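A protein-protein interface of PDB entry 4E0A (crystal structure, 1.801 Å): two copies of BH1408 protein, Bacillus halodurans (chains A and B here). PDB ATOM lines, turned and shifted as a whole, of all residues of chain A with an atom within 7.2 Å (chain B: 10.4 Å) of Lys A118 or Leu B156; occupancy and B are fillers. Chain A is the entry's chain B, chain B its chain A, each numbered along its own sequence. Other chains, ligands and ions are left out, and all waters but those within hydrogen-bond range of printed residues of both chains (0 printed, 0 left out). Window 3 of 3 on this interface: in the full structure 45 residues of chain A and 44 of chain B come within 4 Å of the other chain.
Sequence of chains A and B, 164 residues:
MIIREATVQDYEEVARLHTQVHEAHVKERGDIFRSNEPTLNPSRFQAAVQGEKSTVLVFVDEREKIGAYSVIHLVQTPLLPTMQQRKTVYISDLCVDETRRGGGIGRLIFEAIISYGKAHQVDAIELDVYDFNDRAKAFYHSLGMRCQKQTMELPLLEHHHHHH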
ATOM      1  N   VAL A  89     -16.100  17.666  -3.466  1.00  0.00           N
ATOM      2  CA  VAL A  89     -14.779  17.860  -2.881  1.00  0.00           C
ATOM      3  C   VAL A  89     -13.827  16.969  -3.649  1.00  0.00           C
ATOM      4  O   VAL A  89     -14.036  15.749  -3.741  1.00  0.00           O
ATOM      5  CB  VAL A  89     -14.727  17.471  -1.401  1.00  0.00           C
ATOM      6  CG1 VAL A  89     -13.275  17.479  -0.900  1.00  0.00           C
ATOM      7  CG2 VAL A  89     -15.605  18.409  -0.566  1.00  0.00           C
ATOM      8  N   ALA A 112     -12.381  13.438   8.360  1.00  0.00           N
ATOM      9  CA  ALA A 112     -12.408  14.896   8.425  1.00  0.00           C
ATOM     10  C   ALA A 112     -12.825  15.508   7.084  1.00  0.00           C
ATOM     11  O   ALA A 112     -13.561  16.483   7.060  1.00  0.00           O
ATOM     12  CB  ALA A 112     -11.069  15.446   8.877  1.00  0.00           C
ATOM     13  N   ILE A 113     -12.358  14.932   5.979  1.00  0.00           N
ATOM     14  CA  ILE A 113     -12.747  15.389   4.642  1.00  0.00           C
ATOM     15  C   ILE A 113     -14.253  15.231   4.420  1.00  0.00           C
ATOM     16  O   ILE A 113     -14.916  16.140   3.902  1.00  0.00           O
ATOM     17  CB  ILE A 113     -11.967  14.628   3.548  1.00  0.00           C
ATOM     18  CG1 ILE A 113     -10.481  14.992   3.617  1.00  0.00           C
ATOM     19  CG2 ILE A 113     -12.541  14.918   2.154  1.00  0.00           C
ATOM     20  CD1 ILE A 113      -9.578  14.164   2.682  1.00  0.00           C
ATOM     21  N   ILE A 114     -14.790  14.089   4.848  1.00  0.00           N
ATOM     22  CA  ILE A 114     -16.225  13.844   4.786  1.00  0.00           C
ATOM     23  C   ILE A 114     -17.014  14.907   5.563  1.00  0.00           C
ATOM     24  O   ILE A 114     -17.976  15.466   5.046  1.00  0.00           O
ATOM     25  CB  ILE A 114     -16.569  12.429   5.307  1.00  0.00           C
ATOM     26  CG1 ILE A 114     -16.044  11.368   4.330  1.00  0.00           C
ATOM     27  CG2 ILE A 114     -18.061  12.289   5.524  1.00  0.00           C
ATOM     28  CD1 ILE A 114     -16.143   9.932   4.853  1.00  0.00           C
ATOM     29  N   SER A 115     -16.581  15.178   6.792  1.00  0.00           N
ATOM     30  CA  SER A 115     -17.179  16.203   7.642  1.00  0.00           C
ATOM     31  C   SER A 115     -17.228  17.562   6.938  1.00  0.00           C
ATOM     32  O   SER A 115     -18.254  18.241   6.942  1.00  0.00           O
ATOM     33  CB  SER A 115     -16.394  16.318   8.949  1.00  0.00           C
ATOM     34  OG  SER A 115     -17.029  17.204   9.848  1.00  0.00           O
ATOM     35  N   TYR A 116     -16.108  17.950   6.339  1.00  0.00           N
ATOM     36  CA  TYR A 116     -16.036  19.170   5.535  1.00  0.00           C
ATOM     37  C   TYR A 116     -16.993  19.091   4.336  1.00  0.00           C
ATOM     38  O   TYR A 116     -17.737  20.037   4.047  1.00  0.00           O
ATOM     39  CB  TYR A 116     -14.599  19.367   5.041  1.00  0.00           C
ATOM     40  CG  TYR A 116     -14.410  20.522   4.081  1.00  0.00           C
ATOM     41  CD1 TYR A 116     -14.463  20.324   2.705  1.00  0.00           C
ATOM     42  CD2 TYR A 116     -14.145  21.799   4.550  1.00  0.00           C
ATOM     43  CE1 TYR A 116     -14.282  21.366   1.824  1.00  0.00           C
ATOM     44  CE2 TYR A 116     -13.957  22.857   3.667  1.00  0.00           C
ATOM     45  CZ  TYR A 116     -14.031  22.625   2.308  1.00  0.00           C
ATOM     46  OH  TYR A 116     -13.849  23.658   1.430  1.00  0.00           O
ATOM     47  N   GLY A 117     -16.962  17.962   3.633  1.00  0.00           N
ATOM     48  CA  GLY A 117     -17.814  17.770   2.475  1.00  0.00           C
ATOM     49  C   GLY A 117     -19.289  17.928   2.803  1.00  0.00           C
ATOM     50  O   GLY A 117     -20.025  18.594   2.079  1.00  0.00           O
ATOM     51  N   LYS A 118     -19.722  17.318   3.903  1.00  0.00           N
ATOM     52  CA  LYS A 118     -21.129  17.357   4.289  1.00  0.00           C
ATOM     53  C   LYS A 118     -21.551  18.762   4.711  1.00  0.00           C
ATOM     54  O   LYS A 118     -22.677  19.177   4.462  1.00  0.00           O
ATOM     55  CB  LYS A 118     -21.428  16.361   5.416  1.00  0.00           C
ATOM     56  CG  LYS A 118     -21.406  14.896   5.002  1.00  0.00           C
ATOM     57  CD  LYS A 118     -21.672  14.000   6.207  1.00  0.00           C
ATOM     58  CE  LYS A 118     -21.671  12.519   5.836  1.00  0.00           C
ATOM     59  NZ  LYS A 118     -21.635  11.638   7.048  1.00  0.00           N
ATOM     60  N   ALA A 119     -20.649  19.493   5.358  1.00  0.00           N
ATOM     61  CA  ALA A 119     -20.992  20.829   5.831  1.00  0.00           C
ATOM     62  C   ALA A 119     -21.132  21.778   4.662  1.00  0.00           C
ATOM     63  O   ALA A 119     -21.760  22.821   4.781  1.00  0.00           O
ATOM     64  CB  ALA A 119     -19.962  21.335   6.810  1.00  0.00           C
ATOM     65  N   HIS A 120     -20.567  21.401   3.518  1.00  0.00           N
ATOM     66  CA  HIS A 120     -20.706  22.210   2.300  1.00  0.00           C
ATOM     67  C   HIS A 120     -21.739  21.642   1.323  1.00  0.00           C
ATOM     68  O   HIS A 120     -21.870  22.115   0.199  1.00  0.00           O
ATOM     69  CB  HIS A 120     -19.347  22.416   1.628  1.00  0.00           C
ATOM     70  CG  HIS A 120     -18.447  23.324   2.399  1.00  0.00           C
ATOM     71  ND1 HIS A 120     -17.629  22.873   3.416  1.00  0.00           N
ATOM     72  CD2 HIS A 120     -18.294  24.670   2.358  1.00  0.00           C
ATOM     73  CE1 HIS A 120     -16.988  23.901   3.947  1.00  0.00           C
ATOM     74  NE2 HIS A 120     -17.369  25.001   3.321  1.00  0.00           N
ATOM     75  N   GLN A 121     -22.478  20.636   1.786  1.00  0.00           N
ATOM     76  CA  GLN A 121     -23.540  20.011   1.004  1.00  0.00           C
ATOM     77  C   GLN A 121     -23.077  19.618  -0.413  1.00  0.00           C
ATOM     78  O   GLN A 121     -23.763  19.866  -1.392  1.00  0.00           O
ATOM     79  CB  GLN A 121     -24.782  20.912   0.967  1.00  0.00           C
ATOM     80  CG  GLN A 121     -25.413  21.128   2.340  1.00  0.00           C
ATOM     81  CD  GLN A 121     -25.956  19.836   2.955  1.00  0.00           C
ATOM     82  OE1 GLN A 121     -26.907  19.241   2.451  1.00  0.00           O
ATOM     83  NE2 GLN A 121     -25.349  19.404   4.051  1.00  0.00           N
ATOM     84  N   VAL A 122     -21.905  19.001  -0.505  1.00  0.00           N
ATOM     85  CA  VAL A 122     -21.410  18.545  -1.803  1.00  0.00           C
ATOM     86  C   VAL A 122     -22.093  17.240  -2.213  1.00  0.00           C
ATOM     87  O   VAL A 122     -22.574  16.482  -1.369  1.00  0.00           O
ATOM     88  CB  VAL A 122     -19.881  18.341  -1.801  1.00  0.00           C
ATOM     89  CG1 VAL A 122     -19.175  19.613  -1.326  1.00  0.00           C
ATOM     90  CG2 VAL A 122     -19.506  17.159  -0.933  1.00  0.00           C
ATOM     91  N   ASP A 123     -22.125  16.996  -3.518  1.00  0.00           N
ATOM     92  CA  ASP A 123     -22.707  15.789  -4.084  1.00  0.00           C
ATOM     93  C   ASP A 123     -21.835  14.552  -3.838  1.00  0.00           C
ATOM     94  O   ASP A 123     -22.331  13.455  -3.613  1.00  0.00           O
ATOM     95  CB  ASP A 123     -22.936  16.000  -5.581  1.00  0.00           C
ATOM     96  CG  ASP A 123     -23.880  17.168  -5.860  1.00  0.00           C
ATOM     97  OD1 ASP A 123     -25.053  17.070  -5.458  1.00  0.00           O
ATOM     98  OD2 ASP A 123     -23.455  18.181  -6.453  1.00  0.00           O
ATOM     99  N   ALA A 124     -20.529  14.741  -3.843  1.00  0.00           N
ATOM    100  CA  ALA A 124     -19.627  13.603  -3.713  1.00  0.00           C
ATOM    101  C   ALA A 124     -18.230  14.075  -3.392  1.00  0.00           C
ATOM    102  O   ALA A 124     -17.883  15.233  -3.619  1.00  0.00           O
ATOM    103  CB  ALA A 124     -19.603  12.798  -5.033  1.00  0.00           C
ATOM    104  N   ILE A 125     -17.430  13.158  -2.858  1.00  0.00           N
ATOM    105  CA  ILE A 125     -15.998  13.348  -2.792  1.00  0.00           C
ATOM    106  C   ILE A 125     -15.432  12.590  -3.981  1.00  0.00           C
ATOM    107  O   ILE A 125     -15.878  11.482  -4.263  1.00  0.00           O
ATOM    108  CB  ILE A 125     -15.452  12.739  -1.499  1.00  0.00           C
ATOM    109  CG1 ILE A 125     -15.943  13.569  -0.301  1.00  0.00           C
ATOM    110  CG2 ILE A 125     -13.943  12.668  -1.544  1.00  0.00           C
ATOM    111  CD1 ILE A 125     -15.915  12.814   0.999  1.00  0.00           C
ATOM    112  N   ARG B  29     -26.304   7.312 -15.400  1.00  0.00           N
ATOM    113  CA  ARG B  29     -25.726   8.277 -14.469  1.00  0.00           C
ATOM    114  C   ARG B  29     -26.414   9.629 -14.640  1.00  0.00           C
ATOM    115  O   ARG B  29     -25.787  10.597 -15.080  1.00  0.00           O
ATOM    116  CB  ARG B  29     -24.217   8.435 -14.714  1.00  0.00           C
ATOM    117  CG  ARG B  29     -23.339   7.249 -14.276  1.00  0.00           C
ATOM    118  CD  ARG B  29     -23.565   6.862 -12.818  1.00  0.00           C
ATOM    119  NE  ARG B  29     -23.244   7.924 -11.865  1.00  0.00           N
ATOM    120  CZ  ARG B  29     -22.080   8.044 -11.226  1.00  0.00           C
ATOM    121  NH1 ARG B  29     -21.097   7.181 -11.451  1.00  0.00           N
ATOM    122  NH2 ARG B  29     -21.887   9.046 -10.372  1.00  0.00           N
ATOM    123  N   ASP B  31     -27.176  11.593 -12.476  1.00  0.00           N
ATOM    124  CA  ASP B  31     -26.666  12.529 -11.487  1.00  0.00           C
ATOM    125  C   ASP B  31     -25.565  13.387 -12.090  1.00  0.00           C
ATOM    126  O   ASP B  31     -25.268  14.482 -11.597  1.00  0.00           O
ATOM    127  CB  ASP B  31     -26.179  11.785 -10.227  1.00  0.00           C
ATOM    128  CG  ASP B  31     -25.123  10.739 -10.526  1.00  0.00           C
ATOM    129  OD1 ASP B  31     -25.186  10.079 -11.589  1.00  0.00           O
ATOM    130  OD2 ASP B  31     -24.213  10.569  -9.684  1.00  0.00           O
ATOM    131  N   GLU B 153     -15.241   7.865  -6.540  1.00  0.00           N
ATOM    132  CA  GLU B 153     -16.299   8.722  -6.001  1.00  0.00           C
ATOM    133  C   GLU B 153     -16.949   8.152  -4.744  1.00  0.00           C
ATOM    134  O   GLU B 153     -17.087   6.934  -4.569  1.00  0.00           O
ATOM    135  CB  GLU B 153     -17.388   8.956  -7.055  1.00  0.00           C
ATOM    136  CG  GLU B 153     -18.073   7.688  -7.505  1.00  0.00           C
ATOM    137  CD  GLU B 153     -19.081   7.916  -8.627  1.00  0.00           C
ATOM    138  OE1 GLU B 153     -19.456   9.082  -8.873  1.00  0.00           O
ATOM    139  OE2 GLU B 153     -19.493   6.920  -9.263  1.00  0.00           O
ATOM    140  N   LEU B 154     -17.353   9.055  -3.868  1.00  0.00           N
ATOM    141  CA  LEU B 154     -18.123   8.715  -2.683  1.00  0.00           C
ATOM    142  C   LEU B 154     -19.255   9.720  -2.625  1.00  0.00           C
ATOM    143  O   LEU B 154     -19.040  10.859  -2.214  1.00  0.00           O
ATOM    144  CB  LEU B 154     -17.276   8.843  -1.414  1.00  0.00           C
ATOM    145  CG  LEU B 154     -18.046   8.469  -0.135  1.00  0.00           C
ATOM    146  CD1 LEU B 154     -18.483   7.007  -0.180  1.00  0.00           C
ATOM    147  CD2 LEU B 154     -17.234   8.727   1.107  1.00  0.00           C
ATOM    148  N   PRO B 155     -20.456   9.310  -3.057  1.00  0.00           N
ATOM    149  CA  PRO B 155     -21.625  10.200  -3.027  1.00  0.00           C
ATOM    150  C   PRO B 155     -21.959  10.531  -1.579  1.00  0.00           C
ATOM    151  O   PRO B 155     -21.839   9.657  -0.713  1.00  0.00           O
ATOM    152  CB  PRO B 155     -22.742   9.346  -3.649  1.00  0.00           C
ATOM    153  CG  PRO B 155     -22.053   8.226  -4.349  1.00  0.00           C
ATOM    154  CD  PRO B 155     -20.784   7.976  -3.588  1.00  0.00           C
ATOM    155  N   LEU B 156     -22.333  11.774  -1.305  1.00  0.00           N
ATOM    156  CA  LEU B 156     -22.686  12.166   0.054  1.00  0.00           C
ATOM    157  C   LEU B 156     -24.175  12.452   0.185  1.00  0.00           C
ATOM    158  O   LEU B 156     -24.745  12.339   1.273  1.00  0.00           O
ATOM    159  CB  LEU B 156     -21.874  13.377   0.504  1.00  0.00           C
ATOM    160  CG  LEU B 156     -20.389  13.123   0.770  1.00  0.00           C
ATOM    161  CD1 LEU B 156     -19.758  14.344   1.427  1.00  0.00           C
ATOM    162  CD2 LEU B 156     -20.203  11.879   1.627  1.00  0.00           C
ATOM    163  N   LEU B 157     -24.802  12.811  -0.930  1.00  0.00           N
ATOM    164  CA  LEU B 157     -26.218  13.169  -0.935  1.00  0.00           C
ATOM    165  C   LEU B 157     -27.102  12.015  -1.417  1.00  0.00           C
ATOM    166  O   LEU B 157     -28.007  12.207  -2.234  1.00  0.00           O
ATOM    167  CB  LEU B 157     -26.444  14.414  -1.797  1.00  0.00           C
ATOM    168  CG  LEU B 157     -26.499  15.761  -1.069  1.00  0.00           C
ATOM    169  CD1 LEU B 157     -25.390  15.899  -0.029  1.00  0.00           C
ATOM    170  CD2 LEU B 157     -26.445  16.908  -2.068  1.00  0.00           C
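No position is printed for both chains. Of the 11 pairs that touch across the chains among the printed residues, none has its exchanged pair printed and touching as well.
O of Ile A125 is in hydrogen-bond range of N of Leu B154 (2.9 Å). N of Leu B156 is in hydrogen-bond range of O of Asp A123, at 2.9 Å.
Ala A112 touches none of the printed residues of chain B. Ile A113 touches none of the printed residues of chain B. No residue of chain B comes within 4 Å of Ile A114. Lys A118 touches one residue of chain B. No residue of chain B comes within 4 Å of Ala A119. No residue of chain B comes within 4 Å of Gln A121. Val A122 touches just these residues of chain B: Leu B156 and Leu B157. Of the printed residues of chain B, Asp A123 touches Pro B155, Leu B156 and Leu B157. Printed residues of chain B within 4 Å of Ala A124: Leu B154 and Pro B155. Printed residues of chain B within 4 Å of Ile A125: Glu B153 and Leu B154. Printed residues of chain A within 4 Å of Glu B153: Ile A125 (3.3 Å). Of the printed residues of chain A, Leu B154 touches Ala A124 (3.2 Å) and Ile A125 (2.9 Å). Leu B156 touches just these residues of chain A: Gly A117 (3.9 Å), Lys A118 (3.9 Å), Val A122 (3.7 Å) and Asp A123 (2.9 Å). Of the printed residues of chain A, Leu B157 touches Val A122 and Asp A123. The nearest residue of chain A that does not touch Leu B156 is Ala A124 (4.1 Å).
The guanidinium group (NH1) of Arg B29 lies within salt-bridge range of the side-chain carboxylate (OE2) of Glu B153, at 2.7 Å. N of Val A89 lies within hydrogen-bond range of O of Ala A124. The backbone NH (N) of Val A122 is in hydrogen-bond range of the backbone carbonyl oxygen (O) of Gly A117 (3.2 Å). O of Lys A118 lies within hydrogen-bond range of NE2 of Gln A121.
Among the printed residues, pairs that only touch across the chains: Gly A117 with Leu B156 (3.9 Å), Lys A118 with Leu B156 (3.9 Å), Val A122 with Leu B156 (3.7 Å), Val A122 with Leu B157 (3.2 Å), Asp A123 with Pro B155 (3.4 Å), Asp A123 with Leu B157 (3.7 Å), Ala A124 with Leu B154 (3.2 Å), Ala A124 with Pro B155 (3.9 Å) and Ile A125 with Glu B153 (3.3 Å).
Of the 7 printed residues of chain B, 5 touch a printed residue of chain A. Printed residues of chain B that touch a printed residue of chain A: Glu B153, Leu B154, Pro B155, Leu B156 and Leu B157. Hydrophobic or aromatic side chains of chain B that line the printed part of chain A: Leu B156 and Leu B157. Of the 15 printed residues of chain A, 6 touch a printed residue of chain B. Hydrophobic or aromatic side chains of chain A within 4 Å of the printed part of chain B: Val A122 and Ala A124.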
